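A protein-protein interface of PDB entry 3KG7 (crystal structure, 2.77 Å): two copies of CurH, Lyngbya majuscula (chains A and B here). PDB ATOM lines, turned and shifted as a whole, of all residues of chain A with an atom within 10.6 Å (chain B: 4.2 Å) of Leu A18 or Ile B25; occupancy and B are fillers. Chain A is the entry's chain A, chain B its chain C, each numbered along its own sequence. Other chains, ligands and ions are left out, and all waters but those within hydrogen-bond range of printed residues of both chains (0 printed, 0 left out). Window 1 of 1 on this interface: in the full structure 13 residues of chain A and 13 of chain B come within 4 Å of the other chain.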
ATOM      1  N   ASN A  14      -6.545 -28.559  22.233  1.00  0.00           N
ATOM      2  CA  ASN A  14      -7.888 -28.560  22.809  1.00  0.00           C
ATOM      3  C   ASN A  14      -8.462 -27.175  22.911  1.00  0.00           C
ATOM      4  O   ASN A  14      -7.795 -26.265  23.376  1.00  0.00           O
ATOM      5  CB  ASN A  14      -7.884 -29.177  24.202  1.00  0.00           C
ATOM      6  CG  ASN A  14      -7.488 -30.628  24.188  1.00  0.00           C
ATOM      7  OD1 ASN A  14      -8.141 -31.454  23.549  1.00  0.00           O
ATOM      8  ND2 ASN A  14      -6.413 -30.956  24.896  1.00  0.00           N
ATOM      9  N   LYS A  15      -9.713 -27.032  22.488  1.00  0.00           N
ATOM     10  CA  LYS A  15     -10.425 -25.763  22.524  1.00  0.00           C
ATOM     11  C   LYS A  15     -11.229 -25.642  23.807  1.00  0.00           C
ATOM     12  O   LYS A  15     -11.995 -26.538  24.173  1.00  0.00           O
ATOM     13  CB  LYS A  15     -11.354 -25.651  21.317  1.00  0.00           C
ATOM     14  CG  LYS A  15     -12.102 -24.341  21.198  1.00  0.00           C
ATOM     15  CD  LYS A  15     -13.163 -24.411  20.116  1.00  0.00           C
ATOM     16  CE  LYS A  15     -13.642 -23.015  19.728  1.00  0.00           C
ATOM     17  NZ  LYS A  15     -14.800 -23.047  18.774  1.00  0.00           N
ATOM     18  N   LEU A  16     -11.042 -24.537  24.504  1.00  0.00           N
ATOM     19  CA  LEU A  16     -11.873 -24.231  25.656  1.00  0.00           C
ATOM     20  C   LEU A  16     -12.422 -22.833  25.499  1.00  0.00           C
ATOM     21  O   LEU A  16     -11.670 -21.879  25.264  1.00  0.00           O
ATOM     22  CB  LEU A  16     -11.108 -24.370  26.983  1.00  0.00           C
ATOM     23  CG  LEU A  16     -11.867 -24.156  28.310  1.00  0.00           C
ATOM     24  CD1 LEU A  16     -13.012 -25.168  28.525  1.00  0.00           C
ATOM     25  CD2 LEU A  16     -10.915 -24.231  29.472  1.00  0.00           C
ATOM     26  N   GLU A  17     -13.740 -22.727  25.608  1.00  0.00           N
ATOM     27  CA  GLU A  17     -14.406 -21.435  25.563  1.00  0.00           C
ATOM     28  C   GLU A  17     -14.667 -20.964  26.979  1.00  0.00           C
ATOM     29  O   GLU A  17     -15.289 -21.673  27.775  1.00  0.00           O
ATOM     30  CB  GLU A  17     -15.725 -21.512  24.814  1.00  0.00           C
ATOM     31  CG  GLU A  17     -15.595 -21.704  23.339  1.00  0.00           C
ATOM     32  CD  GLU A  17     -16.940 -21.904  22.683  1.00  0.00           C
ATOM     33  OE1 GLU A  17     -17.192 -21.250  21.645  1.00  0.00           O
ATOM     34  OE2 GLU A  17     -17.748 -22.711  23.208  1.00  0.00           O
ATOM     35  N   LEU A  18     -14.191 -19.761  27.293  1.00  0.00           N
ATOM     36  CA  LEU A  18     -14.353 -19.209  28.642  1.00  0.00           C
ATOM     37  C   LEU A  18     -15.734 -18.637  28.839  1.00  0.00           C
ATOM     38  O   LEU A  18     -16.192 -17.794  28.076  1.00  0.00           O
ATOM     39  CB  LEU A  18     -13.277 -18.173  28.977  1.00  0.00           C
ATOM     40  CG  LEU A  18     -11.942 -18.735  29.490  1.00  0.00           C
ATOM     41  CD1 LEU A  18     -11.164 -19.480  28.436  1.00  0.00           C
ATOM     42  CD2 LEU A  18     -11.097 -17.608  29.998  1.00  0.00           C
ATOM     43  N   ALA A  19     -16.401 -19.137  29.866  1.00  0.00           N
ATOM     44  CA  ALA A  19     -17.748 -18.726  30.216  1.00  0.00           C
ATOM     45  C   ALA A  19     -17.799 -17.251  30.533  1.00  0.00           C
ATOM     46  O   ALA A  19     -18.710 -16.532  30.117  1.00  0.00           O
ATOM     47  CB  ALA A  19     -18.208 -19.502  31.441  1.00  0.00           C
ATOM     48  N   SER A  20     -16.806 -16.812  31.293  1.00  0.00           N
ATOM     49  CA  SER A  20     -16.841 -15.504  31.928  1.00  0.00           C
ATOM     50  C   SER A  20     -16.581 -14.347  30.966  1.00  0.00           C
ATOM     51  O   SER A  20     -17.231 -13.303  31.063  1.00  0.00           O
ATOM     52  CB  SER A  20     -15.865 -15.452  33.114  1.00  0.00           C
ATOM     53  OG  SER A  20     -14.525 -15.526  32.675  1.00  0.00           O
ATOM     54  N   THR A  21     -15.652 -14.542  30.035  1.00  0.00           N
ATOM     55  CA  THR A  21     -15.183 -13.451  29.191  1.00  0.00           C
ATOM     56  C   THR A  21     -15.545 -13.572  27.712  1.00  0.00           C
ATOM     57  O   THR A  21     -15.499 -12.581  26.984  1.00  0.00           O
ATOM     58  CB  THR A  21     -13.671 -13.348  29.232  1.00  0.00           C
ATOM     59  OG1 THR A  21     -13.122 -14.528  28.634  1.00  0.00           O
ATOM     60  CG2 THR A  21     -13.165 -13.196  30.675  1.00  0.00           C
ATOM     61  N   GLY A  22     -15.877 -14.778  27.261  1.00  0.00           N
ATOM     62  CA  GLY A  22     -16.058 -15.046  25.835  1.00  0.00           C
ATOM     63  C   GLY A  22     -14.727 -15.163  25.107  1.00  0.00           C
ATOM     64  O   GLY A  22     -14.648 -14.933  23.907  1.00  0.00           O
ATOM     65  N   GLN A  23     -13.668 -15.515  25.833  1.00  0.00           N
ATOM     66  CA  GLN A  23     -12.379 -15.794  25.213  1.00  0.00           C
ATOM     67  C   GLN A  23     -12.266 -17.272  24.852  1.00  0.00           C
ATOM     68  O   GLN A  23     -13.045 -18.102  25.326  1.00  0.00           O
ATOM     69  CB  GLN A  23     -11.238 -15.399  26.143  1.00  0.00           C
ATOM     70  CG  GLN A  23     -11.112 -13.908  26.393  1.00  0.00           C
ATOM     71  CD  GLN A  23     -10.460 -13.591  27.731  1.00  0.00           C
ATOM     72  OE1 GLN A  23     -10.606 -14.340  28.705  1.00  0.00           O
ATOM     73  NE2 GLN A  23      -9.751 -12.471  27.793  1.00  0.00           N
ATOM     74  N   THR A  24     -11.291 -17.596  24.010  1.00  0.00           N
ATOM     75  CA  THR A  24     -11.041 -18.977  23.658  1.00  0.00           C
ATOM     76  C   THR A  24      -9.571 -19.300  23.856  1.00  0.00           C
ATOM     77  O   THR A  24      -8.704 -18.559  23.413  1.00  0.00           O
ATOM     78  CB  THR A  24     -11.495 -19.281  22.238  1.00  0.00           C
ATOM     79  OG1 THR A  24     -12.834 -18.813  22.088  1.00  0.00           O
ATOM     80  CG2 THR A  24     -11.481 -20.783  21.982  1.00  0.00           C
ATOM     81  N   ILE A  25      -9.318 -20.409  24.543  1.00  0.00           N
ATOM     82  CA  ILE A  25      -7.982 -20.917  24.780  1.00  0.00           C
ATOM     83  C   ILE A  25      -7.783 -22.218  24.011  1.00  0.00           C
ATOM     84  O   ILE A  25      -8.585 -23.131  24.123  1.00  0.00           O
ATOM     85  CB  ILE A  25      -7.792 -21.212  26.295  1.00  0.00           C
ATOM     86  CG1 ILE A  25      -7.578 -19.922  27.067  1.00  0.00           C
ATOM     87  CG2 ILE A  25      -6.610 -22.160  26.548  1.00  0.00           C
ATOM     88  CD1 ILE A  25      -6.140 -19.459  27.021  1.00  0.00           C
ATOM     89  N   TYR A  26      -6.706 -22.297  23.246  1.00  0.00           N
ATOM     90  CA  TYR A  26      -6.284 -23.553  22.660  1.00  0.00           C
ATOM     91  C   TYR A  26      -5.045 -24.007  23.385  1.00  0.00           C
ATOM     92  O   TYR A  26      -4.012 -23.308  23.382  1.00  0.00           O
ATOM     93  CB  TYR A  26      -6.013 -23.388  21.178  1.00  0.00           C
ATOM     94  CG  TYR A  26      -7.266 -23.008  20.434  1.00  0.00           C
ATOM     95  CD1 TYR A  26      -8.120 -23.981  19.927  1.00  0.00           C
ATOM     96  CD2 TYR A  26      -7.621 -21.666  20.280  1.00  0.00           C
ATOM     97  CE1 TYR A  26      -9.268 -23.624  19.264  1.00  0.00           C
ATOM     98  CE2 TYR A  26      -8.763 -21.312  19.625  1.00  0.00           C
ATOM     99  CZ  TYR A  26      -9.576 -22.284  19.121  1.00  0.00           C
ATOM    100  OH  TYR A  26     -10.714 -21.901  18.468  1.00  0.00           O
ATOM    101  N   HIS A  27      -5.140 -25.161  24.037  1.00  0.00           N
ATOM    102  CA  HIS A  27      -4.009 -25.655  24.811  1.00  0.00           C
ATOM    103  C   HIS A  27      -3.592 -27.060  24.430  1.00  0.00           C
ATOM    104  O   HIS A  27      -4.424 -27.941  24.214  1.00  0.00           O
ATOM    105  CB  HIS A  27      -4.284 -25.553  26.304  1.00  0.00           C
ATOM    106  CG  HIS A  27      -5.460 -26.355  26.758  1.00  0.00           C
ATOM    107  ND1 HIS A  27      -5.345 -27.649  27.217  1.00  0.00           N
ATOM    108  CD2 HIS A  27      -6.773 -26.040  26.842  1.00  0.00           C
ATOM    109  CE1 HIS A  27      -6.539 -28.098  27.564  1.00  0.00           C
ATOM    110  NE2 HIS A  27      -7.421 -27.140  27.347  1.00  0.00           N
ATOM    111  N   GLU A  87       4.094 -27.057  27.650  1.00  0.00           N
ATOM    112  CA  GLU A  87       2.660 -26.818  27.620  1.00  0.00           C
ATOM    113  C   GLU A  87       2.397 -25.436  27.036  1.00  0.00           C
ATOM    114  O   GLU A  87       2.887 -24.425  27.527  1.00  0.00           O
ATOM    115  CB  GLU A  87       1.970 -27.065  28.975  1.00  0.00           C
ATOM    116  CG  GLU A  87       2.175 -26.031  30.062  1.00  0.00           C
ATOM    117  CD  GLU A  87       1.209 -26.211  31.228  1.00  0.00           C
ATOM    118  OE1 GLU A  87       1.659 -26.567  32.343  1.00  0.00           O
ATOM    119  OE2 GLU A  87      -0.004 -26.004  31.031  1.00  0.00           O
ATOM    120  N   GLN A  89      -0.186 -22.432  25.176  1.00  0.00           N
ATOM    121  CA  GLN A  89      -1.529 -21.847  25.146  1.00  0.00           C
ATOM    122  C   GLN A  89      -1.603 -20.731  24.129  1.00  0.00           C
ATOM    123  O   GLN A  89      -0.784 -19.808  24.162  1.00  0.00           O
ATOM    124  CB  GLN A  89      -1.915 -21.302  26.511  1.00  0.00           C
ATOM    125  CG  GLN A  89      -2.008 -22.359  27.593  1.00  0.00           C
ATOM    126  CD  GLN A  89      -2.472 -21.787  28.915  1.00  0.00           C
ATOM    127  OE1 GLN A  89      -2.852 -20.610  28.994  1.00  0.00           O
ATOM    128  NE2 GLN A  89      -2.443 -22.612  29.967  1.00  0.00           N
ATOM    129  N   LEU A  90      -2.563 -20.832  23.208  1.00  0.00           N
ATOM    130  CA  LEU A  90      -2.897 -19.725  22.306  1.00  0.00           C
ATOM    131  C   LEU A  90      -4.190 -19.130  22.815  1.00  0.00           C
ATOM    132  O   LEU A  90      -5.203 -19.815  22.916  1.00  0.00           O
ATOM    133  CB  LEU A  90      -3.048 -20.192  20.856  1.00  0.00           C
ATOM    134  CG  LEU A  90      -3.291 -19.152  19.736  1.00  0.00           C
ATOM    135  CD1 LEU A  90      -2.959 -19.712  18.361  1.00  0.00           C
ATOM    136  CD2 LEU A  90      -4.716 -18.584  19.723  1.00  0.00           C
ATOM    137  N   MET A  91      -4.153 -17.851  23.153  1.00  0.00           N
ATOM    138  CA  MET A  91      -5.308 -17.169  23.731  1.00  0.00           C
ATOM    139  C   MET A  91      -5.942 -16.217  22.706  1.00  0.00           C
ATOM    140  O   MET A  91      -5.311 -15.258  22.247  1.00  0.00           O
ATOM    141  CB  MET A  91      -4.891 -16.452  25.022  1.00  0.00           C
ATOM    142  CG  MET A  91      -5.883 -15.444  25.564  1.00  0.00           C
ATOM    143  SD  MET A  91      -7.186 -16.167  26.821  1.00  0.00           S
ATOM    144  CE  MET A  91      -6.124 -16.129  28.454  1.00  0.00           C
ATOM    145  N   LEU A  92      -7.180 -16.525  22.321  1.00  0.00           N
ATOM    146  CA  LEU A  92      -7.941 -15.689  21.390  1.00  0.00           C
ATOM    147  C   LEU A  92      -8.912 -14.809  22.177  1.00  0.00           C
ATOM    148  O   LEU A  92      -9.909 -15.286  22.738  1.00  0.00           O
ATOM    149  CB  LEU A  92      -8.671 -16.534  20.349  1.00  0.00           C
ATOM    150  CG  LEU A  92      -9.605 -15.830  19.346  1.00  0.00           C
ATOM    151  CD1 LEU A  92      -8.832 -15.137  18.219  1.00  0.00           C
ATOM    152  CD2 LEU A  92     -10.620 -16.810  18.760  1.00  0.00           C
ATOM    153  N   HIS A  93      -8.594 -13.517  22.231  1.00  0.00           N
ATOM    154  CA  HIS A  93      -9.359 -12.577  23.035  1.00  0.00           C
ATOM    155  C   HIS A  93     -10.715 -12.311  22.419  1.00  0.00           C
ATOM    156  O   HIS A  93     -10.908 -12.481  21.216  1.00  0.00           O
ATOM    157  CB  HIS A  93      -8.573 -11.280  23.244  1.00  0.00           C
ATOM    158  CG  HIS A  93      -7.443 -11.425  24.215  1.00  0.00           C
ATOM    159  ND1 HIS A  93      -7.503 -10.948  25.507  1.00  0.00           N
ATOM    160  CD2 HIS A  93      -6.237 -12.031  24.094  1.00  0.00           C
ATOM    161  CE1 HIS A  93      -6.380 -11.239  26.137  1.00  0.00           C
ATOM    162  NE2 HIS A  93      -5.594 -11.896  25.301  1.00  0.00           N
ATOM    163  N   THR A  94     -11.665 -11.927  23.256  1.00  0.00           N
ATOM    164  CA  THR A  94     -12.980 -11.562  22.769  1.00  0.00           C
ATOM    165  C   THR A  94     -12.864 -10.251  21.993  1.00  0.00           C
ATOM    166  O   THR A  94     -12.091  -9.365  22.364  1.00  0.00           O
ATOM    167  CB  THR A  94     -14.031 -11.487  23.899  1.00  0.00           C
ATOM    168  OG1 THR A  94     -15.239 -10.930  23.378  1.00  0.00           O
ATOM    169  CG2 THR A  94     -13.544 -10.630  25.064  1.00  0.00           C
ATOM    170  N   ARG A 108       5.255 -22.815  28.787  1.00  0.00           N
ATOM    171  CA  ARG A 108       6.204 -23.067  29.873  1.00  0.00           C
ATOM    172  C   ARG A 108       6.590 -24.532  29.840  1.00  0.00           C
ATOM    173  O   ARG A 108       5.886 -25.346  29.251  1.00  0.00           O
ATOM    174  CB  ARG A 108       5.596 -22.726  31.236  1.00  0.00           C
ATOM    175  CG  ARG A 108       4.351 -23.505  31.580  1.00  0.00           C
ATOM    176  CD  ARG A 108       3.954 -23.272  32.992  1.00  0.00           C
ATOM    177  NE  ARG A 108       2.793 -24.081  33.322  1.00  0.00           N
ATOM    178  CZ  ARG A 108       1.985 -23.848  34.349  1.00  0.00           C
ATOM    179  NH1 ARG A 108       2.212 -22.821  35.159  1.00  0.00           N
ATOM    180  NH2 ARG A 108       0.941 -24.640  34.553  1.00  0.00           N
ATOM    181  N   TRP A 116       5.697 -18.685  32.693  1.00  0.00           N
ATOM    182  CA  TRP A 116       5.228 -18.629  31.310  1.00  0.00           C
ATOM    183  C   TRP A 116       6.059 -17.647  30.494  1.00  0.00           C
ATOM    184  O   TRP A 116       6.346 -16.538  30.940  1.00  0.00           O
ATOM    185  CB  TRP A 116       3.749 -18.233  31.220  1.00  0.00           C
ATOM    186  CG  TRP A 116       2.753 -19.196  31.797  1.00  0.00           C
ATOM    187  CD1 TRP A 116       2.170 -19.122  33.025  1.00  0.00           C
ATOM    188  CD2 TRP A 116       2.192 -20.352  31.159  1.00  0.00           C
ATOM    189  NE1 TRP A 116       1.287 -20.159  33.202  1.00  0.00           N
ATOM    190  CE2 TRP A 116       1.278 -20.930  32.073  1.00  0.00           C
ATOM    191  CE3 TRP A 116       2.374 -20.960  29.909  1.00  0.00           C
ATOM    192  CZ2 TRP A 116       0.555 -22.092  31.782  1.00  0.00           C
ATOM    193  CZ3 TRP A 116       1.641 -22.112  29.615  1.00  0.00           C
ATOM    194  CH2 TRP A 116       0.750 -22.666  30.554  1.00  0.00           C
ATOM    195  N   ASN B  14     -11.151 -30.503  35.635  1.00  0.00           N
ATOM    196  CA  ASN B  14      -9.850 -30.220  35.056  1.00  0.00           C
ATOM    197  C   ASN B  14      -9.345 -28.840  35.400  1.00  0.00           C
ATOM    198  O   ASN B  14     -10.086 -27.870  35.293  1.00  0.00           O
ATOM    199  CB  ASN B  14      -9.927 -30.349  33.542  1.00  0.00           C
ATOM    200  CG  ASN B  14     -10.280 -31.726  33.107  1.00  0.00           C
ATOM    201  OD1 ASN B  14      -9.411 -32.578  32.937  1.00  0.00           O
ATOM    202  ND2 ASN B  14     -11.567 -31.963  32.914  1.00  0.00           N
ATOM    203  N   LYS B  15      -8.069 -28.764  35.761  1.00  0.00           N
ATOM    204  CA  LYS B  15      -7.417 -27.519  36.127  1.00  0.00           C
ATOM    205  C   LYS B  15      -6.706 -26.922  34.922  1.00  0.00           C
ATOM    206  O   LYS B  15      -5.898 -27.598  34.276  1.00  0.00           O
ATOM    207  CB  LYS B  15      -6.397 -27.795  37.240  1.00  0.00           C
ATOM    208  CG  LYS B  15      -5.846 -26.556  37.896  1.00  0.00           C
ATOM    209  CD  LYS B  15      -4.640 -26.838  38.764  1.00  0.00           C
ATOM    210  CE  LYS B  15      -4.356 -25.635  39.653  1.00  0.00           C
ATOM    211  NZ  LYS B  15      -3.091 -25.722  40.431  1.00  0.00           N
ATOM    212  N   LEU B  16      -6.999 -25.659  34.621  1.00  0.00           N
ATOM    213  CA  LEU B  16      -6.267 -24.940  33.585  1.00  0.00           C
ATOM    214  C   LEU B  16      -5.763 -23.615  34.117  1.00  0.00           C
ATOM    215  O   LEU B  16      -6.542 -22.810  34.602  1.00  0.00           O
ATOM    216  CB  LEU B  16      -7.132 -24.727  32.342  1.00  0.00           C
ATOM    217  CG  LEU B  16      -6.373 -24.388  31.054  1.00  0.00           C
ATOM    218  CD1 LEU B  16      -5.390 -25.480  30.667  1.00  0.00           C
ATOM    219  CD2 LEU B  16      -7.358 -24.153  29.927  1.00  0.00           C
ATOM    220  N   LEU B  18      -4.223 -20.065  33.245  1.00  0.00           N
ATOM    221  CA  LEU B  18      -4.204 -19.167  32.104  1.00  0.00           C
ATOM    222  C   LEU B  18      -2.922 -18.382  32.053  1.00  0.00           C
ATOM    223  O   LEU B  18      -2.558 -17.693  32.996  1.00  0.00           O
ATOM    224  CB  LEU B  18      -5.441 -18.275  32.094  1.00  0.00           C
ATOM    225  CG  LEU B  18      -6.711 -19.120  31.963  1.00  0.00           C
ATOM    226  CD1 LEU B  18      -7.898 -18.231  31.752  1.00  0.00           C
ATOM    227  CD2 LEU B  18      -6.584 -20.128  30.815  1.00  0.00           C
ATOM    228  N   THR B  24      -7.156 -19.214  37.011  1.00  0.00           N
ATOM    229  CA  THR B  24      -7.280 -20.657  37.027  1.00  0.00           C
ATOM    230  C   THR B  24      -8.730 -21.024  36.744  1.00  0.00           C
ATOM    231  O   THR B  24      -9.653 -20.498  37.379  1.00  0.00           O
ATOM    232  CB  THR B  24      -6.873 -21.214  38.400  1.00  0.00           C
ATOM    233  OG1 THR B  24      -5.584 -20.703  38.755  1.00  0.00           O
ATOM    234  CG2 THR B  24      -6.793 -22.724  38.374  1.00  0.00           C
ATOM    235  N   ILE B  25      -8.938 -21.902  35.768  1.00  0.00           N
ATOM    236  CA  ILE B  25     -10.282 -22.401  35.477  1.00  0.00           C
ATOM    237  C   ILE B  25     -10.326 -23.861  35.839  1.00  0.00           C
ATOM    238  O   ILE B  25      -9.442 -24.617  35.456  1.00  0.00           O
ATOM    239  CB  ILE B  25     -10.695 -22.283  33.983  1.00  0.00           C
ATOM    240  CG1 ILE B  25     -10.451 -20.886  33.441  1.00  0.00           C
ATOM    241  CG2 ILE B  25     -12.180 -22.610  33.792  1.00  0.00           C
ATOM    242  CD1 ILE B  25     -10.527 -20.827  31.926  1.00  0.00           C
ATOM    243  N   TYR B  26     -11.359 -24.245  36.581  1.00  0.00           N
ATOM    244  CA  TYR B  26     -11.678 -25.637  36.791  1.00  0.00           C
ATOM    245  C   TYR B  26     -12.928 -25.987  35.988  1.00  0.00           C
ATOM    246  O   TYR B  26     -14.021 -25.485  36.261  1.00  0.00           O
ATOM    247  CB  TYR B  26     -11.877 -25.905  38.271  1.00  0.00           C
ATOM    248  CG  TYR B  26     -10.661 -25.592  39.124  1.00  0.00           C
ATOM    249  CD1 TYR B  26      -9.739 -26.596  39.460  1.00  0.00           C
ATOM    250  CD2 TYR B  26     -10.435 -24.293  39.610  1.00  0.00           C
ATOM    251  CE1 TYR B  26      -8.622 -26.319  40.245  1.00  0.00           C
ATOM    252  CE2 TYR B  26      -9.314 -24.007  40.402  1.00  0.00           C
ATOM    253  CZ  TYR B  26      -8.418 -25.026  40.714  1.00  0.00           C
ATOM    254  OH  TYR B  26      -7.312 -24.755  41.493  1.00  0.00           O
ATOM    255  N   HIS B  27     -12.764 -26.831  34.976  1.00  0.00           N
ATOM    256  CA  HIS B  27     -13.878 -27.152  34.096  1.00  0.00           C
ATOM    257  C   HIS B  27     -14.201 -28.632  34.074  1.00  0.00           C
ATOM    258  O   HIS B  27     -13.300 -29.466  34.032  1.00  0.00           O
ATOM    259  CB  HIS B  27     -13.630 -26.611  32.689  1.00  0.00           C
ATOM    260  CG  HIS B  27     -12.443 -27.204  32.004  1.00  0.00           C
ATOM    261  ND1 HIS B  27     -12.559 -28.125  30.983  1.00  0.00           N
ATOM    262  CD2 HIS B  27     -11.115 -26.995  32.176  1.00  0.00           C
ATOM    263  CE1 HIS B  27     -11.354 -28.459  30.555  1.00  0.00           C
ATOM    264  NE2 HIS B  27     -10.460 -27.790  31.263  1.00  0.00           N
ATOM    265  N   GLN B  89     -17.977 -24.331  34.876  1.00  0.00           N
ATOM    266  CA  GLN B  89     -16.685 -23.662  34.985  1.00  0.00           C
ATOM    267  C   GLN B  89     -16.610 -22.850  36.262  1.00  0.00           C
ATOM    268  O   GLN B  89     -17.455 -21.982  36.497  1.00  0.00           O
ATOM    269  CB  GLN B  89     -16.438 -22.752  33.781  1.00  0.00           C
ATOM    270  CG  GLN B  89     -16.120 -23.498  32.496  1.00  0.00           C
ATOM    271  CD  GLN B  89     -15.564 -22.606  31.403  1.00  0.00           C
ATOM    272  OE1 GLN B  89     -15.357 -21.412  31.605  1.00  0.00           O
ATOM    273  NE2 GLN B  89     -15.322 -23.184  30.233  1.00  0.00           N
ATOM    274  N   LEU B  90     -15.616 -23.155  37.096  1.00  0.00           N
ATOM    275  CA  LEU B  90     -15.316 -22.344  38.271  1.00  0.00           C
ATOM    276  C   LEU B  90     -14.088 -21.518  37.931  1.00  0.00           C
ATOM    277  O   LEU B  90     -13.030 -22.073  37.611  1.00  0.00           O
ATOM    278  CB  LEU B  90     -15.060 -23.225  39.492  1.00  0.00           C
ATOM    279  CG  LEU B  90     -14.804 -22.520  40.828  1.00  0.00           C
ATOM    280  CD1 LEU B  90     -15.218 -23.403  42.000  1.00  0.00           C
ATOM    281  CD2 LEU B  90     -13.340 -22.094  40.970  1.00  0.00           C
ATOM    282  N   MET B  91     -14.233 -20.199  37.982  1.00  0.00           N
ATOM    283  CA  MET B  91     -13.168 -19.290  37.598  1.00  0.00           C
ATOM    284  C   MET B  91     -12.564 -18.628  38.842  1.00  0.00           C
ATOM    285  O   MET B  91     -13.252 -17.929  39.597  1.00  0.00           O
ATOM    286  CB  MET B  91     -13.716 -18.272  36.592  1.00  0.00           C
ATOM    287  CG  MET B  91     -12.760 -17.158  36.160  1.00  0.00           C
ATOM    288  SD  MET B  91     -11.320 -17.710  34.940  1.00  0.00           S
ATOM    289  CE  MET B  91     -11.533 -16.279  33.615  1.00  0.00           C
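O of Asn A14 sits at hydrogen-bond distance from N of His A27 (3.0 Å). The backbone carbonyl oxygen (O) of Ile A25 sits at hydrogen-bond distance from the backbone NH (N) of Leu A16, at 2.9 Å. N of Leu A18 sits at hydrogen-bond distance from O of Gln A23, at 2.8 Å. The backbone NH of Asn B14 is in hydrogen-bond range of the backbone carbonyl oxygen of His B27 (2.9 Å). O of Ile B25 is in hydrogen-bond range of N of Leu B16, at 2.8 Å.
Leu A16 touches Leu B16 (CD2 to CD2, 3.6 Å). Leu A16 touches His B27. Gln B89 touches Leu A16 (NE2 to CD1, 3.5 Å). Leu A18 touches Leu B18 (CD2 to CD1, 3.7 Å). Ile B25 touches Leu A18. CA of Leu A18 touches OE1 of Gln B89, at 3.8 Å. CD2 of Leu A18 touches CE of Met B91, at 3.9 Å. OG of Ser A20 touches CE of Met B91, at 3.2 Å. Ile A25 touches Leu B18 (CD1 to CD2, 3.9 Å). His A27 touches Leu B16 (CD2 to CD2, 3.7 Å).
The backbone carbonyl oxygen (O) of Glu A17 lies within hydrogen-bond range of the side-chain amide nitrogen (NE2) of Gln B89, 2.9 Å away. N of Ala A19 is in hydrogen-bond range of OE1 of Gln B89, at 3.0 Å.
Leu A16 touches Gln B89, but with the chains exchanged Gln A89 does not touch Leu B16 (4.2 Å). Leu A18 touches Gln B89, and with the chains exchanged Gln A89 touches Leu B18. Leu A18 touches Met B91, but with the chains exchanged Met A91 does not touch Leu B18 (4.3 Å). Ile A25 touches Leu B16, but with the chains exchanged Leu A16 does not touch Ile B25 (4.2 Å).
Printed residues of chain A within 4 Å of Ile B25: Leu A18. Printed residues of chain B within 4 Å of Leu A16: Leu B16 (3.6 Å), His B27 (3.9 Å) and Gln B89 (3.5 Å). Of the printed residues of chain B, His A27 touches Leu B16 (3.7 Å). Of the printed residues of chain B, Ala A19 touches Gln B89. Of the printed residues of chain B, Gln A89 touches Leu B18. Of the printed residues of chain A, Met B91 touches Leu A18 (3.9 Å) and Ser A20 (3.2 Å). The nearest residue of chain A that does not touch Ile B25 is Leu A16 (4.2 Å).
Of the 11 printed residues of chain B, 6 touch a printed residue of chain A. Hydrophobic or aromatic side chains of chain B that line the printed part of chain A: Leu B16, Leu B18, Ile B25, His B27 and Met B91. Of the 23 printed residues of chain A, 8 touch a printed residue of chain B.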
